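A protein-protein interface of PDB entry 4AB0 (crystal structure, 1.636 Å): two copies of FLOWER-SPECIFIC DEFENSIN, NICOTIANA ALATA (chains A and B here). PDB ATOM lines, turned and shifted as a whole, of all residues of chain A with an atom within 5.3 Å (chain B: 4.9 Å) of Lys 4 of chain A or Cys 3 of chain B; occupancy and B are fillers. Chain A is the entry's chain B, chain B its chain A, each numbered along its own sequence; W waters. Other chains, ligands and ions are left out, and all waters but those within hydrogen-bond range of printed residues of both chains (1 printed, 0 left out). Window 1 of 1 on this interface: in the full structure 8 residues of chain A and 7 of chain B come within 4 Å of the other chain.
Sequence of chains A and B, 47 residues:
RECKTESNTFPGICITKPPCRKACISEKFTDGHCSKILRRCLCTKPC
O of Lys 4 of chain B is in hydrogen-bond range of N of Lys 4 of chain A. OG1 of Thr 5 of chain B lies close to SG of Cys 3 of chain A.
Cys 3 of chain A touches Lys 4 of chain B, and with the chains exchanged Lys 4 of chain A touches Cys 3 of chain B. Cys 3 of chain A touches Thr 5 of chain B, and with the chains exchanged Thr 5 of chain A touches Cys 3 of chain B. Lys 4 of chain A touches Glu 2 of chain B, but with the chains exchanged Glu 2 of chain A does not touch Lys 4 of chain B (4.2 Å). Lys 4 of chain B touches its own counterpart, Lys 4 of chain A. Positions printed for both chains: 2, 3, 4, 5, 43 and 44.
Of the printed residues of chain B, Lys 4 of chain A touches Glu 2, Cys 3 and Lys 4. Cys 3 of chain B touches just these residues of chain A: Lys 4 (3.3 Å), Thr 5 (3.98 Å) and Leu 42 (3.8 Å). Of the printed residues of chain B, Cys 3 of chain A touches Lys 4 and Thr 5. Of the printed residues of chain A, Thr 5 of chain B touches Cys 3. Thr 44 of chain B touches none of the printed residues of chain A. Cys 43 of chain B touches none of the printed residues of chain A. The nearest printed residue of chain A that does not touch Lys 4 of chain B is Glu 2 of chain A (4.2 Å).
Water W1 lies within hydrogen-bond range of OG1 of Thr 5 of chain A, N of Glu 6 of chain A and SG of Cys 47 of chain B.
Of the 9 printed residues of chain A, 4 touch a printed residue of chain B. Printed residues of chain A that touch a printed residue of chain B: Cys 3, Lys 4, Thr 5 and Leu 42. Along chain A the printed residues that touch a printed residue of chain B span positions 3 to 42. Of the 9 printed residues of chain B, 6 touch a printed residue of chain A. Printed residues of chain B that touch a printed residue of chain A: Glu 2, Cys 3, Lys 4, Thr 5, Phe 29 and Cys 47. Hydrophobic or aromatic side chains of chain B within 4 Å of the printed part of chain A: Phe 29. Among the printed residues, 9 pairs touch across the chains. Among the printed residues, no Asp or Glu carboxylate lies within 4 Å of a Lys or Arg side-chain nitrogen of the other chain.
O of Lys 45 of chain B is in hydrogen-bond range of N of Cys 3 of chain B, at 2.9 Å. The side-chain sulfur of Cys 3 of chain B forms a disulfide with the side-chain sulfur of Cys 47 of chain B, 2.0 Å away. The backbone carbonyl oxygen (O) of Thr 5 of chain B lies within hydrogen-bond range of the backbone NH (N) of Cys 43 of chain B, at 2.7 Å. N of Cys 43 of chain A sits at hydrogen-bond distance from O of Thr 5 of chain A, at 2.8 Å. O of His 33 of chain A is in hydrogen-bond range of N of Leu 42 of chain A (2.8 Å).
Among the printed residues, merely in contact across the chains: Cys 3 of chain A with Lys 4 of chain B, Lys 4 of chain A with Glu 2 of chain B, Lys 4 of chain A with Cys 3 of chain B, Thr 5 of chain A with Cys 3 of chain B, Thr 5 of chain A with Phe 29 of chain B, Leu 42 of chain A with Cys 3 of chain B and Leu 42 of chain A with Cys 47 of chain B.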
ATOM      1  N   GLU A   2      18.407  -0.559   9.363  1.00  0.00           N
ATOM      2  CA  GLU A   2      18.491   0.887   9.179  1.00  0.00           C
ATOM      3  C   GLU A   2      17.097   1.459   9.018  1.00  0.00           C
ATOM      4  O   GLU A   2      16.305   0.981   8.204  1.00  0.00           O
ATOM      5  CB  GLU A   2      19.336   1.276   7.965  1.00  0.00           C
ATOM      6  CG  GLU A   2      19.479   2.788   7.812  1.00  0.00           C
ATOM      7  CD  GLU A   2      20.376   3.182   6.656  1.00  0.00           C
ATOM      8  OE1 GLU A   2      19.889   3.212   5.505  1.00  0.00           O
ATOM      9  OE2 GLU A   2      21.569   3.464   6.902  1.00  0.00           O
ATOM     10  N   CYS A   3      16.804   2.484   9.809  1.00  0.00           N
ATOM     11  CA  CYS A   3      15.546   3.208   9.700  1.00  0.00           C
ATOM     12  C   CYS A   3      15.771   4.442   8.837  1.00  0.00           C
ATOM     13  O   CYS A   3      16.810   5.093   8.940  1.00  0.00           O
ATOM     14  CB  CYS A   3      15.036   3.605  11.088  1.00  0.00           C
ATOM     15  SG  CYS A   3      14.217   2.257  11.993  1.00  0.00           S
ATOM     16  N   LYS A   4      14.801   4.746   7.978  1.00  0.00           N
ATOM     17  CA  LYS A   4      14.896   5.881   7.070  1.00  0.00           C
ATOM     18  C   LYS A   4      13.544   6.571   6.982  1.00  0.00           C
ATOM     19  O   LYS A   4      12.532   5.951   6.651  1.00  0.00           O
ATOM     20  CB  LYS A   4      15.341   5.433   5.677  1.00  0.00           C
ATOM     21  CG  LYS A   4      15.414   6.563   4.664  1.00  0.00           C
ATOM     22  CD  LYS A   4      16.185   6.147   3.416  1.00  0.00           C
ATOM     23  CE  LYS A   4      15.329   5.318   2.471  1.00  0.00           C
ATOM     24  NZ  LYS A   4      16.077   4.920   1.243  1.00  0.00           N
ATOM     25  N   THR A   5      13.525   7.857   7.295  1.00  0.00           N
ATOM     26  CA  THR A   5      12.275   8.590   7.318  1.00  0.00           C
ATOM     27  C   THR A   5      12.551  10.065   7.084  1.00  0.00           C
ATOM     28  O   THR A   5      13.658  10.545   7.323  1.00  0.00           O
ATOM     29  CB  THR A   5      11.536   8.372   8.656  1.00  0.00           C
ATOM     30  OG1 THR A   5      10.187   8.835   8.545  1.00  0.00           O
ATOM     31  CG2 THR A   5      12.242   9.093   9.798  1.00  0.00           C
ATOM     32  N   GLU A   6      11.548  10.779   6.592  1.00  0.00           N
ATOM     33  CA  GLU A   6      11.729  12.178   6.247  1.00  0.00           C
ATOM     34  C   GLU A   6      12.018  13.010   7.490  1.00  0.00           C
ATOM     35  O   GLU A   6      11.425  12.791   8.552  1.00  0.00           O
ATOM     36  CB  GLU A   6      10.486  12.717   5.532  1.00  0.00           C
ATOM     37  CG  GLU A   6      10.592  14.183   5.160  1.00  0.00           C
ATOM     38  CD  GLU A   6       9.438  14.664   4.299  1.00  0.00           C
ATOM     39  OE1 GLU A   6       8.361  14.023   4.306  1.00  0.00           O
ATOM     40  OE2 GLU A   6       9.616  15.690   3.617  1.00  0.00           O
ATOM     41  N   HIS A  33      20.221  12.622   3.763  1.00  0.00           N
ATOM     42  CA  HIS A  33      20.490  12.798   2.338  1.00  0.00           C
ATOM     43  C   HIS A  33      19.220  13.230   1.612  1.00  0.00           C
ATOM     44  O   HIS A  33      18.112  13.039   2.117  1.00  0.00           O
ATOM     45  CB  HIS A  33      20.968  11.487   1.728  1.00  0.00           C
ATOM     46  CG  HIS A  33      19.991  10.371   1.889  1.00  0.00           C
ATOM     47  ND1 HIS A  33      19.117   9.996   0.887  1.00  0.00           N
ATOM     48  CD2 HIS A  33      19.721   9.563   2.938  1.00  0.00           C
ATOM     49  CE1 HIS A  33      18.364   8.998   1.317  1.00  0.00           C
ATOM     50  NE2 HIS A  33      18.716   8.714   2.559  1.00  0.00           N
ATOM     51  N   LEU A  42      15.867  13.054   3.817  1.00  0.00           N
ATOM     52  CA  LEU A  42      15.620  11.768   4.457  1.00  0.00           C
ATOM     53  C   LEU A  42      16.703  11.468   5.482  1.00  0.00           C
ATOM     54  O   LEU A  42      17.895  11.537   5.179  1.00  0.00           O
ATOM     55  CB  LEU A  42      15.585  10.651   3.414  1.00  0.00           C
ATOM     56  CG  LEU A  42      14.588  10.858   2.270  1.00  0.00           C
ATOM     57  CD1 LEU A  42      14.528   9.621   1.386  1.00  0.00           C
ATOM     58  CD2 LEU A  42      13.210  11.218   2.813  1.00  0.00           C
ATOM     59  N   CYS A  43      16.279  11.127   6.694  1.00  0.00           N
ATOM     60  CA  CYS A  43      17.204  10.820   7.779  1.00  0.00           C
ATOM     61  C   CYS A  43      17.381   9.321   7.927  1.00  0.00           C
ATOM     62  O   CYS A  43      16.448   8.554   7.695  1.00  0.00           O
ATOM     63  CB  CYS A  43      16.678  11.383   9.094  1.00  0.00           C
ATOM     64  SG  CYS A  43      16.327  13.139   9.038  1.00  0.00           S
ATOM     65  N   THR A  44      18.577   8.909   8.326  1.00  0.00           N
ATOM     66  CA  THR A  44      18.874   7.496   8.511  1.00  0.00           C
ATOM     67  C   THR A  44      19.560   7.285   9.852  1.00  0.00           C
ATOM     68  O   THR A  44      20.299   8.149  10.323  1.00  0.00           O
ATOM     69  CB  THR A  44      19.786   6.953   7.386  1.00  0.00           C
ATOM     70  OG1 THR A  44      20.942   7.791   7.251  1.00  0.00           O
ATOM     71  CG2 THR A  44      19.046   6.909   6.057  1.00  0.00           C
ATOM     72  N   GLU B   2      12.056   3.241  -0.754  1.00  0.00           N
ATOM     73  CA  GLU B   2      11.057   3.870   0.101  1.00  0.00           C
ATOM     74  C   GLU B   2      11.609   4.178   1.481  1.00  0.00           C
ATOM     75  O   GLU B   2      12.642   3.648   1.890  1.00  0.00           O
ATOM     76  CB  GLU B   2       9.833   2.962   0.256  1.00  0.00           C
ATOM     77  CG  GLU B   2      10.162   1.499   0.509  1.00  0.00           C
ATOM     78  CD  GLU B   2       8.939   0.608   0.420  1.00  0.00           C
ATOM     79  OE1 GLU B   2       7.887   1.089  -0.053  1.00  0.00           O
ATOM     80  OE2 GLU B   2       9.026  -0.571   0.825  1.00  0.00           O
ATOM     81  N   CYS B   3      10.905   5.045   2.196  1.00  0.00           N
ATOM     82  CA  CYS B   3      11.152   5.215   3.619  1.00  0.00           C
ATOM     83  C   CYS B   3      10.605   4.012   4.356  1.00  0.00           C
ATOM     84  O   CYS B   3       9.574   3.452   3.982  1.00  0.00           O
ATOM     85  CB  CYS B   3      10.503   6.489   4.135  1.00  0.00           C
ATOM     86  SG  CYS B   3      11.312   7.960   3.511  1.00  0.00           S
ATOM     87  N   LYS B   4      11.310   3.621   5.408  1.00  0.00           N
ATOM     88  CA  LYS B   4      10.933   2.464   6.198  1.00  0.00           C
ATOM     89  C   LYS B   4      11.427   2.693   7.606  1.00  0.00           C
ATOM     90  O   LYS B   4      12.621   2.878   7.834  1.00  0.00           O
ATOM     91  CB  LYS B   4      11.556   1.187   5.639  1.00  0.00           C
ATOM     92  CG  LYS B   4      11.015  -0.073   6.294  1.00  0.00           C
ATOM     93  CD  LYS B   4      11.657  -1.331   5.736  1.00  0.00           C
ATOM     94  CE  LYS B   4      12.825  -1.790   6.591  1.00  0.00           C
ATOM     95  NZ  LYS B   4      13.274  -3.161   6.221  1.00  0.00           N
ATOM     96  N   THR B   5      10.508   2.694   8.557  1.00  0.00           N
ATOM     97  CA  THR B   5      10.900   2.900   9.932  1.00  0.00           C
ATOM     98  C   THR B   5       9.862   2.298  10.851  1.00  0.00           C
ATOM     99  O   THR B   5       8.768   1.943  10.419  1.00  0.00           O
ATOM    100  CB  THR B   5      11.075   4.394  10.239  1.00  0.00           C
ATOM    101  OG1 THR B   5      11.867   4.550  11.421  1.00  0.00           O
ATOM    102  CG2 THR B   5       9.727   5.078  10.429  1.00  0.00           C
ATOM    103  N   PHE B  29       2.111   7.117   6.512  1.00  0.00           N
ATOM    104  CA  PHE B  29       2.761   6.190   5.598  1.00  0.00           C
ATOM    105  C   PHE B  29       1.681   5.530   4.745  1.00  0.00           C
ATOM    106  O   PHE B  29       0.495   5.820   4.915  1.00  0.00           O
ATOM    107  CB  PHE B  29       3.545   5.144   6.383  1.00  0.00           C
ATOM    108  CG  PHE B  29       4.699   5.716   7.147  1.00  0.00           C
ATOM    109  CD1 PHE B  29       4.506   6.281   8.398  1.00  0.00           C
ATOM    110  CD2 PHE B  29       5.975   5.710   6.607  1.00  0.00           C
ATOM    111  CE1 PHE B  29       5.561   6.819   9.100  1.00  0.00           C
ATOM    112  CE2 PHE B  29       7.042   6.242   7.307  1.00  0.00           C
ATOM    113  CZ  PHE B  29       6.834   6.800   8.554  1.00  0.00           C
ATOM    114  N   CYS B  43       6.671   0.743   9.151  1.00  0.00           N
ATOM    115  CA  CYS B  43       5.887   1.543   8.215  1.00  0.00           C
ATOM    116  C   CYS B  43       6.699   1.850   6.963  1.00  0.00           C
ATOM    117  O   CYS B  43       7.907   2.055   7.049  1.00  0.00           O
ATOM    118  CB  CYS B  43       5.472   2.861   8.865  1.00  0.00           C
ATOM    119  SG  CYS B  43       4.508   2.706  10.379  1.00  0.00           S
ATOM    120  N   THR B  44       6.026   1.899   5.814  1.00  0.00           N
ATOM    121  CA  THR B  44       6.675   2.215   4.542  1.00  0.00           C
ATOM    122  C   THR B  44       5.882   3.231   3.735  1.00  0.00           C
ATOM    123  O   THR B  44       4.651   3.285   3.805  1.00  0.00           O
ATOM    124  CB  THR B  44       6.862   0.962   3.654  1.00  0.00           C
ATOM    125  OG1 THR B  44       5.608   0.293   3.478  1.00  0.00           O
ATOM    126  CG2 THR B  44       7.857   0.005   4.273  1.00  0.00           C
ATOM    127  N   LYS B  45       6.599   4.038   2.962  1.00  0.00           N
ATOM    128  CA  LYS B  45       5.968   4.950   2.022  1.00  0.00           C
ATOM    129  C   LYS B  45       6.958   5.374   0.971  1.00  0.00           C
ATOM    130  O   LYS B  45       8.168   5.312   1.192  1.00  0.00           O
ATOM    131  CB  LYS B  45       5.453   6.205   2.730  1.00  0.00           C
ATOM    132  CG  LYS B  45       6.555   7.152   3.197  1.00  0.00           C
ATOM    133  CD  LYS B  45       5.985   8.339   3.960  1.00  0.00           C
ATOM    134  CE  LYS B  45       5.373   9.369   3.024  1.00  0.00           C
ATOM    135  NZ  LYS B  45       4.821  10.530   3.772  1.00  0.00           N
ATOM    136  N   CYS B  47       9.560   8.183  -0.865  1.00  0.00           N
ATOM    137  CA  CYS B  47      10.090   9.277  -0.079  1.00  0.00           C
ATOM    138  C   CYS B  47      11.117   9.964  -0.960  1.00  0.00           C
ATOM    139  O   CYS B  47      11.684   9.321  -1.840  1.00  0.00           O
ATOM    140  CB  CYS B  47      10.712   8.737   1.216  1.00  0.00           C
ATOM    141  SG  CYS B  47       9.653   8.800   2.673  1.00  0.00           S
ATOM    142  OXT CYS B  47      11.379  11.161  -0.863  1.00  0.00           O
HETATM  143  O   HOH W   1       8.909   9.631   6.299  1.00  0.00           O
